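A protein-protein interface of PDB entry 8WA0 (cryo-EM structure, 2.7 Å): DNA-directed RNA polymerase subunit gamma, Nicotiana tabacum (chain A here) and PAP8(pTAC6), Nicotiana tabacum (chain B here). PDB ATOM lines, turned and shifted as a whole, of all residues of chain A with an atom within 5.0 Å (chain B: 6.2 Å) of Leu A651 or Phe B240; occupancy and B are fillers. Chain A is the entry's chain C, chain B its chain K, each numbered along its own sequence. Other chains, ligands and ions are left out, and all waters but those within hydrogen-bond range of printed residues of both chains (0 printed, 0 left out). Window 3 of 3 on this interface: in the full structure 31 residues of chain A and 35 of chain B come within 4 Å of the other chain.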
ATOM      1  N   TYR A 632     -22.021 -11.754 -12.195  1.00  0.00           N
ATOM      2  CA  TYR A 632     -21.356 -11.562 -10.895  1.00  0.00           C
ATOM      3  C   TYR A 632     -21.283 -12.835 -10.133  1.00  0.00           C
ATOM      4  O   TYR A 632     -22.285 -13.477  -9.962  1.00  0.00           O
ATOM      5  CB  TYR A 632     -22.171 -10.573 -10.103  1.00  0.00           C
ATOM      6  CG  TYR A 632     -21.481  -9.729  -9.076  1.00  0.00           C
ATOM      7  CD1 TYR A 632     -20.280 -10.108  -8.511  1.00  0.00           C
ATOM      8  CD2 TYR A 632     -22.065  -8.551  -8.647  1.00  0.00           C
ATOM      9  CE1 TYR A 632     -19.666  -9.324  -7.561  1.00  0.00           C
ATOM     10  CE2 TYR A 632     -21.464  -7.767  -7.696  1.00  0.00           C
ATOM     11  CZ  TYR A 632     -20.265  -8.158  -7.158  1.00  0.00           C
ATOM     12  OH  TYR A 632     -19.655  -7.379  -6.210  1.00  0.00           O
ATOM     13  N   SER A 634     -20.150 -15.396  -6.692  1.00  0.00           N
ATOM     14  CA  SER A 634     -20.172 -15.339  -5.222  1.00  0.00           C
ATOM     15  C   SER A 634     -18.909 -15.019  -4.487  1.00  0.00           C
ATOM     16  O   SER A 634     -18.937 -14.268  -3.534  1.00  0.00           O
ATOM     17  CB  SER A 634     -20.680 -16.637  -4.693  1.00  0.00           C
ATOM     18  OG  SER A 634     -19.819 -17.685  -5.076  1.00  0.00           O
ATOM     19  N   LEU A 635     -17.795 -15.553  -4.893  1.00  0.00           N
ATOM     20  CA  LEU A 635     -16.560 -15.164  -4.281  1.00  0.00           C
ATOM     21  C   LEU A 635     -16.223 -13.691  -4.522  1.00  0.00           C
ATOM     22  O   LEU A 635     -15.447 -13.122  -3.773  1.00  0.00           O
ATOM     23  CB  LEU A 635     -15.457 -16.114  -4.695  1.00  0.00           C
ATOM     24  CG  LEU A 635     -13.989 -15.866  -4.340  1.00  0.00           C
ATOM     25  CD1 LEU A 635     -13.350 -17.129  -3.784  1.00  0.00           C
ATOM     26  CD2 LEU A 635     -13.218 -15.354  -5.549  1.00  0.00           C
ATOM     27  N   GLY A 636     -16.776 -13.050  -5.541  1.00  0.00           N
ATOM     28  CA  GLY A 636     -16.581 -11.624  -5.740  1.00  0.00           C
ATOM     29  C   GLY A 636     -16.166 -10.981  -7.036  1.00  0.00           C
ATOM     30  O   GLY A 636     -16.232  -9.772  -7.134  1.00  0.00           O
ATOM     31  N   ARG A 649     -13.415  -7.190 -13.012  1.00  0.00           N
ATOM     32  CA  ARG A 649     -13.109  -6.477 -11.795  1.00  0.00           C
ATOM     33  C   ARG A 649     -13.272  -7.382 -10.584  1.00  0.00           C
ATOM     34  O   ARG A 649     -13.864  -8.430 -10.700  1.00  0.00           O
ATOM     35  CB  ARG A 649     -13.957  -5.241 -11.730  1.00  0.00           C
ATOM     36  CG  ARG A 649     -13.345  -4.093 -12.482  1.00  0.00           C
ATOM     37  CD  ARG A 649     -13.927  -2.785 -12.026  1.00  0.00           C
ATOM     38  NE  ARG A 649     -15.267  -2.633 -12.538  1.00  0.00           N
ATOM     39  CZ  ARG A 649     -15.968  -1.520 -12.433  1.00  0.00           C
ATOM     40  NH1 ARG A 649     -15.447  -0.462 -11.833  1.00  0.00           N
ATOM     41  NH2 ARG A 649     -17.186  -1.463 -12.936  1.00  0.00           N
ATOM     42  N   SER A 650     -12.720  -7.021  -9.435  1.00  0.00           N
ATOM     43  CA  SER A 650     -12.735  -7.857  -8.232  1.00  0.00           C
ATOM     44  C   SER A 650     -13.251  -7.161  -7.024  1.00  0.00           C
ATOM     45  O   SER A 650     -13.628  -6.012  -7.110  1.00  0.00           O
ATOM     46  CB  SER A 650     -11.351  -8.306  -7.912  1.00  0.00           C
ATOM     47  OG  SER A 650     -10.461  -7.207  -7.929  1.00  0.00           O
ATOM     48  N   LEU A 651     -13.316  -7.843  -5.893  1.00  0.00           N
ATOM     49  CA  LEU A 651     -13.927  -7.267  -4.694  1.00  0.00           C
ATOM     50  C   LEU A 651     -13.251  -6.038  -4.192  1.00  0.00           C
ATOM     51  O   LEU A 651     -13.888  -5.111  -3.736  1.00  0.00           O
ATOM     52  CB  LEU A 651     -14.070  -8.286  -3.586  1.00  0.00           C
ATOM     53  CG  LEU A 651     -15.207  -8.040  -2.597  1.00  0.00           C
ATOM     54  CD1 LEU A 651     -16.546  -8.017  -3.311  1.00  0.00           C
ATOM     55  CD2 LEU A 651     -15.197  -9.106  -1.525  1.00  0.00           C
ATOM     56  N   LYS A 652     -11.960  -5.989  -4.320  1.00  0.00           N
ATOM     57  CA  LYS A 652     -11.244  -4.813  -3.942  1.00  0.00           C
ATOM     58  C   LYS A 652     -11.531  -3.671  -4.928  1.00  0.00           C
ATOM     59  O   LYS A 652     -10.964  -2.591  -4.766  1.00  0.00           O
ATOM     60  CB  LYS A 652      -9.768  -5.133  -3.920  1.00  0.00           C
ATOM     61  CG  LYS A 652      -9.372  -6.215  -4.902  1.00  0.00           C
ATOM     62  CD  LYS A 652      -8.128  -6.952  -4.437  1.00  0.00           C
ATOM     63  CE  LYS A 652      -7.905  -8.207  -5.265  1.00  0.00           C
ATOM     64  NZ  LYS A 652      -9.081  -9.116  -5.201  1.00  0.00           N
ATOM     65  N   LYS A 653     -12.368  -3.894  -5.953  1.00  0.00           N
ATOM     66  CA  LYS A 653     -12.694  -2.878  -6.996  1.00  0.00           C
ATOM     67  C   LYS A 653     -11.529  -2.442  -7.839  1.00  0.00           C
ATOM     68  O   LYS A 653     -11.337  -1.269  -8.104  1.00  0.00           O
ATOM     69  CB  LYS A 653     -13.448  -1.672  -6.418  1.00  0.00           C
ATOM     70  CG  LYS A 653     -14.955  -1.733  -6.613  1.00  0.00           C
ATOM     71  CD  LYS A 653     -15.599  -2.795  -5.738  1.00  0.00           C
ATOM     72  CE  LYS A 653     -15.637  -2.362  -4.281  1.00  0.00           C
ATOM     73  NZ  LYS A 653     -16.367  -3.345  -3.434  1.00  0.00           N
ATOM     74  N   ALA B 193     -21.209  -5.204   0.066  1.00  0.00           N
ATOM     75  CA  ALA B 193     -20.180  -4.889  -0.905  1.00  0.00           C
ATOM     76  C   ALA B 193     -20.716  -3.943  -1.977  1.00  0.00           C
ATOM     77  O   ALA B 193     -21.834  -4.134  -2.427  1.00  0.00           O
ATOM     78  CB  ALA B 193     -19.748  -6.146  -1.565  1.00  0.00           C
ATOM     79  N   MET B 194     -19.956  -2.933  -2.399  1.00  0.00           N
ATOM     80  CA  MET B 194     -20.437  -1.966  -3.386  1.00  0.00           C
ATOM     81  C   MET B 194     -19.875  -2.051  -4.810  1.00  0.00           C
ATOM     82  O   MET B 194     -18.712  -2.288  -4.992  1.00  0.00           O
ATOM     83  CB  MET B 194     -20.359  -0.536  -2.866  1.00  0.00           C
ATOM     84  CG  MET B 194     -19.032   0.148  -3.095  1.00  0.00           C
ATOM     85  SD  MET B 194     -19.189   1.932  -2.993  1.00  0.00           S
ATOM     86  CE  MET B 194     -19.150   2.182  -1.223  1.00  0.00           C
ATOM     87  N   HIS B 229     -23.488  -9.395   2.515  1.00  0.00           N
ATOM     88  CA  HIS B 229     -22.597 -10.490   2.673  1.00  0.00           C
ATOM     89  C   HIS B 229     -23.463 -11.530   3.366  1.00  0.00           C
ATOM     90  O   HIS B 229     -24.385 -11.165   4.077  1.00  0.00           O
ATOM     91  CB  HIS B 229     -21.359 -10.122   3.473  1.00  0.00           C
ATOM     92  CG  HIS B 229     -20.370  -9.278   2.756  1.00  0.00           C
ATOM     93  ND1 HIS B 229     -19.060  -9.188   3.163  1.00  0.00           N
ATOM     94  CD2 HIS B 229     -20.485  -8.478   1.673  1.00  0.00           C
ATOM     95  CE1 HIS B 229     -18.406  -8.371   2.361  1.00  0.00           C
ATOM     96  NE2 HIS B 229     -19.248  -7.928   1.446  1.00  0.00           N
ATOM     97  N   TYR B 230     -23.200 -12.816   3.181  1.00  0.00           N
ATOM     98  CA  TYR B 230     -24.042 -13.855   3.749  1.00  0.00           C
ATOM     99  C   TYR B 230     -23.833 -13.980   5.194  1.00  0.00           C
ATOM    100  O   TYR B 230     -22.698 -14.121   5.624  1.00  0.00           O
ATOM    101  CB  TYR B 230     -23.661 -15.195   3.174  1.00  0.00           C
ATOM    102  CG  TYR B 230     -24.663 -16.293   3.369  1.00  0.00           C
ATOM    103  CD1 TYR B 230     -26.015 -16.062   3.202  1.00  0.00           C
ATOM    104  CD2 TYR B 230     -24.253 -17.573   3.683  1.00  0.00           C
ATOM    105  CE1 TYR B 230     -26.934 -17.074   3.372  1.00  0.00           C
ATOM    106  CE2 TYR B 230     -25.164 -18.589   3.852  1.00  0.00           C
ATOM    107  CZ  TYR B 230     -26.502 -18.331   3.694  1.00  0.00           C
ATOM    108  OH  TYR B 230     -27.415 -19.342   3.861  1.00  0.00           O
ATOM    109  N   ARG B 233     -21.081 -12.364   7.313  1.00  0.00           N
ATOM    110  CA  ARG B 233     -19.761 -12.927   7.469  1.00  0.00           C
ATOM    111  C   ARG B 233     -18.715 -12.023   6.876  1.00  0.00           C
ATOM    112  O   ARG B 233     -19.052 -11.065   6.197  1.00  0.00           O
ATOM    113  CB  ARG B 233     -19.696 -14.334   6.902  1.00  0.00           C
ATOM    114  CG  ARG B 233     -20.291 -15.383   7.818  1.00  0.00           C
ATOM    115  CD  ARG B 233     -20.565 -16.680   7.083  1.00  0.00           C
ATOM    116  NE  ARG B 233     -20.881 -17.766   8.005  1.00  0.00           N
ATOM    117  CZ  ARG B 233     -21.286 -18.973   7.628  1.00  0.00           C
ATOM    118  NH1 ARG B 233     -21.439 -19.250   6.340  1.00  0.00           N
ATOM    119  NH2 ARG B 233     -21.548 -19.900   8.537  1.00  0.00           N
ATOM    120  N   ARG B 234     -17.447 -12.301   7.103  1.00  0.00           N
ATOM    121  CA  ARG B 234     -16.408 -11.389   6.679  1.00  0.00           C
ATOM    122  C   ARG B 234     -15.548 -11.988   5.639  1.00  0.00           C
ATOM    123  O   ARG B 234     -15.442 -13.195   5.549  1.00  0.00           O
ATOM    124  CB  ARG B 234     -15.541 -11.040   7.875  1.00  0.00           C
ATOM    125  CG  ARG B 234     -14.635  -9.835   7.702  1.00  0.00           C
ATOM    126  CD  ARG B 234     -13.658  -9.732   8.859  1.00  0.00           C
ATOM    127  NE  ARG B 234     -14.340  -9.546  10.134  1.00  0.00           N
ATOM    128  CZ  ARG B 234     -14.573  -8.362  10.688  1.00  0.00           C
ATOM    129  NH1 ARG B 234     -14.173  -7.252  10.083  1.00  0.00           N
ATOM    130  NH2 ARG B 234     -15.200  -8.286  11.854  1.00  0.00           N
ATOM    131  N   ALA B 235     -14.915 -11.159   4.838  1.00  0.00           N
ATOM    132  CA  ALA B 235     -14.144 -11.646   3.711  1.00  0.00           C
ATOM    133  C   ALA B 235     -13.145 -12.684   4.039  1.00  0.00           C
ATOM    134  O   ALA B 235     -12.963 -13.625   3.269  1.00  0.00           O
ATOM    135  CB  ALA B 235     -13.465 -10.492   3.011  1.00  0.00           C
ATOM    136  N   GLY B 236     -12.480 -12.549   5.159  1.00  0.00           N
ATOM    137  CA  GLY B 236     -11.418 -13.468   5.454  1.00  0.00           C
ATOM    138  C   GLY B 236     -11.878 -14.878   5.653  1.00  0.00           C
ATOM    139  O   GLY B 236     -11.155 -15.807   5.320  1.00  0.00           O
ATOM    140  N   ASP B 237     -13.073 -15.063   6.179  1.00  0.00           N
ATOM    141  CA  ASP B 237     -13.515 -16.392   6.529  1.00  0.00           C
ATOM    142  C   ASP B 237     -13.530 -17.312   5.384  1.00  0.00           C
ATOM    143  O   ASP B 237     -13.826 -16.917   4.260  1.00  0.00           O
ATOM    144  CB  ASP B 237     -14.923 -16.331   7.084  1.00  0.00           C
ATOM    145  CG  ASP B 237     -15.037 -15.419   8.283  1.00  0.00           C
ATOM    146  OD1 ASP B 237     -13.993 -15.100   8.894  1.00  0.00           O
ATOM    147  OD2 ASP B 237     -16.171 -15.024   8.625  1.00  0.00           O
ATOM    148  N   PRO B 238     -13.235 -18.563   5.645  1.00  0.00           N
ATOM    149  CA  PRO B 238     -13.350 -19.518   4.565  1.00  0.00           C
ATOM    150  C   PRO B 238     -14.754 -19.545   4.028  1.00  0.00           C
ATOM    151  O   PRO B 238     -14.912 -19.738   2.836  1.00  0.00           O
ATOM    152  CB  PRO B 238     -13.037 -20.825   5.246  1.00  0.00           C
ATOM    153  CG  PRO B 238     -12.071 -20.459   6.318  1.00  0.00           C
ATOM    154  CD  PRO B 238     -12.495 -19.102   6.794  1.00  0.00           C
ATOM    155  N   GLU B 239     -15.756 -19.388   4.857  1.00  0.00           N
ATOM    156  CA  GLU B 239     -17.124 -19.305   4.384  1.00  0.00           C
ATOM    157  C   GLU B 239     -17.599 -17.923   3.934  1.00  0.00           C
ATOM    158  O   GLU B 239     -18.429 -17.330   4.600  1.00  0.00           O
ATOM    159  CB  GLU B 239     -18.058 -19.765   5.488  1.00  0.00           C
ATOM    160  N   PHE B 240     -17.131 -17.423   2.792  1.00  0.00           N
ATOM    161  CA  PHE B 240     -17.596 -16.135   2.278  1.00  0.00           C
ATOM    162  C   PHE B 240     -18.394 -16.304   1.035  1.00  0.00           C
ATOM    163  O   PHE B 240     -18.025 -17.061   0.156  1.00  0.00           O
ATOM    164  CB  PHE B 240     -16.464 -15.160   2.020  1.00  0.00           C
ATOM    165  CG  PHE B 240     -16.905 -13.853   1.459  1.00  0.00           C
ATOM    166  CD1 PHE B 240     -17.768 -13.050   2.160  1.00  0.00           C
ATOM    167  CD2 PHE B 240     -16.437 -13.425   0.241  1.00  0.00           C
ATOM    168  CE1 PHE B 240     -18.177 -11.845   1.646  1.00  0.00           C
ATOM    169  CE2 PHE B 240     -16.840 -12.222  -0.284  1.00  0.00           C
ATOM    170  CZ  PHE B 240     -17.709 -11.426   0.423  1.00  0.00           C
ATOM    171  N   ALA B 241     -19.500 -15.608   0.963  1.00  0.00           N
ATOM    172  CA  ALA B 241     -20.341 -15.703  -0.163  1.00  0.00           C
ATOM    173  C   ALA B 241     -21.154 -14.493  -0.055  1.00  0.00           C
ATOM    174  O   ALA B 241     -20.990 -13.719   0.864  1.00  0.00           O
ATOM    175  CB  ALA B 241     -21.202 -16.925  -0.068  1.00  0.00           C
ATOM    176  N   LEU B 242     -22.001 -14.275  -1.015  1.00  0.00           N
ATOM    177  CA  LEU B 242     -22.762 -13.095  -1.016  1.00  0.00           C
ATOM    178  C   LEU B 242     -24.161 -13.530  -1.179  1.00  0.00           C
ATOM    179  O   LEU B 242     -24.419 -14.518  -1.836  1.00  0.00           O
ATOM    180  CB  LEU B 242     -22.310 -12.228  -2.161  1.00  0.00           C
ATOM    181  CG  LEU B 242     -20.915 -11.624  -2.279  1.00  0.00           C
ATOM    182  CD1 LEU B 242     -20.653 -11.193  -3.709  1.00  0.00           C
ATOM    183  CD2 LEU B 242     -20.794 -10.434  -1.357  1.00  0.00           C
ATOM    184  N   ARG B 274     -24.444 -21.631  -1.875  1.00  0.00           N
ATOM    185  CA  ARG B 274     -24.103 -20.314  -2.341  1.00  0.00           C
ATOM    186  C   ARG B 274     -22.734 -20.294  -2.961  1.00  0.00           C
ATOM    187  O   ARG B 274     -22.234 -19.234  -3.286  1.00  0.00           O
ATOM    188  CB  ARG B 274     -24.240 -19.338  -1.213  1.00  0.00           C
ATOM    189  CG  ARG B 274     -25.549 -19.459  -0.457  1.00  0.00           C
ATOM    190  CD  ARG B 274     -26.635 -18.615  -1.087  1.00  0.00           C
ATOM    191  NE  ARG B 274     -27.825 -18.566  -0.248  1.00  0.00           N
ATOM    192  CZ  ARG B 274     -28.858 -17.761  -0.464  1.00  0.00           C
ATOM    193  NH1 ARG B 274     -28.847 -16.927  -1.495  1.00  0.00           N
ATOM    194  NH2 ARG B 274     -29.899 -17.782   0.354  1.00  0.00           N
ATOM    195  N   LYS B 275     -22.103 -21.447  -3.120  1.00  0.00           N
ATOM    196  CA  LYS B 275     -20.835 -21.493  -3.843  1.00  0.00           C
ATOM    197  C   LYS B 275     -20.975 -21.817  -5.314  1.00  0.00           C
ATOM    198  O   LYS B 275     -19.994 -21.849  -6.032  1.00  0.00           O
ATOM    199  CB  LYS B 275     -19.868 -22.457  -3.184  1.00  0.00           C
ATOM    200  CG  LYS B 275     -19.072 -21.849  -2.040  1.00  0.00           C
ATOM    201  CD  LYS B 275     -18.103 -20.786  -2.539  1.00  0.00           C
ATOM    202  CE  LYS B 275     -18.540 -19.386  -2.140  1.00  0.00           C
ATOM    203  NZ  LYS B 275     -17.632 -18.340  -2.684  1.00  0.00           N
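O of Ala B241 sits at hydrogen-bond distance from N of Tyr B230, 3.3 Å away. NZ of Lys B275 lies within hydrogen-bond range of O of Phe B240 (3.1 Å). The backbone carbonyl oxygen of Leu A651 is in hydrogen-bond range of the side-chain amino group of Lys A653, 3.1 Å away.
The backbone carbonyl oxygen (O) of Met B194 lies within hydrogen-bond range of the side-chain amino group (NZ) of Lys A653, 3.0 Å away. The backbone carbonyl oxygen (O) of Arg B274 lies close to the side-chain hydroxyl (OG) of Ser A634 (3.4 Å). The side-chain amino group of Lys B275 sits at hydrogen-bond distance from the side-chain hydroxyl of Ser A634, 3.3 Å away.
Ser A634 touches Ala B241. Leu B242 touches Ser A634 (CD1 to O, 3.5 Å). Leu A635 touches Phe B240 (O to CE2, 3.9 Å). NZ of Lys B275 touches N of Leu A635 (3.6 Å). Leu A651 touches Phe B240 (CD2 to CE2, 3.7 Å).
Of the printed residues of chain B, Ser A634 touches Ala B241 (3.9 Å), Leu B242 (3.5 Å), Arg B274 (3.3 Å) and Lys B275 (3.3 Å). Printed residues of chain B within 4 Å of Leu A635: Phe B240 (3.9 Å) and Lys B275 (3.6 Å). Of chain B, only Phe B240 (3.7 Å) comes within 4 Å of Leu A651. Printed residues of chain B within 4 Å of Lys A653: Met B194 (3.0 Å). Tyr B230 touches none of the printed residues of chain A. Printed residues of chain A within 4 Å of Arg B274: Ser A634. The nearest residue of chain B that does not touch Leu A651 is Ala B193 (4.1 Å). The nearest residue of chain A that does not touch Phe B240 is Ser A634 (4.4 Å). The nearest printed residue of chain A that does not touch Ala B241 is Leu A635 (5.4 Å).
Of the 16 printed residues of chain B, 6 touch a printed residue of chain A. Printed residues of chain B that touch a printed residue of chain A: Met B194, Phe B240, Ala B241, Leu B242, Arg B274 and Lys B275. Hydrophobic or aromatic side chains of chain B within 4 Å of the printed part of chain A: Phe B240 and Leu B242. Hydrophobic or aromatic side chains of chain A within 4 Å of the printed part of chain B: Leu A635 and Leu A651. Among the printed residues, no Asp or Glu carboxylate lies within 4 Å of a Lys or Arg side-chain nitrogen of the other chain.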
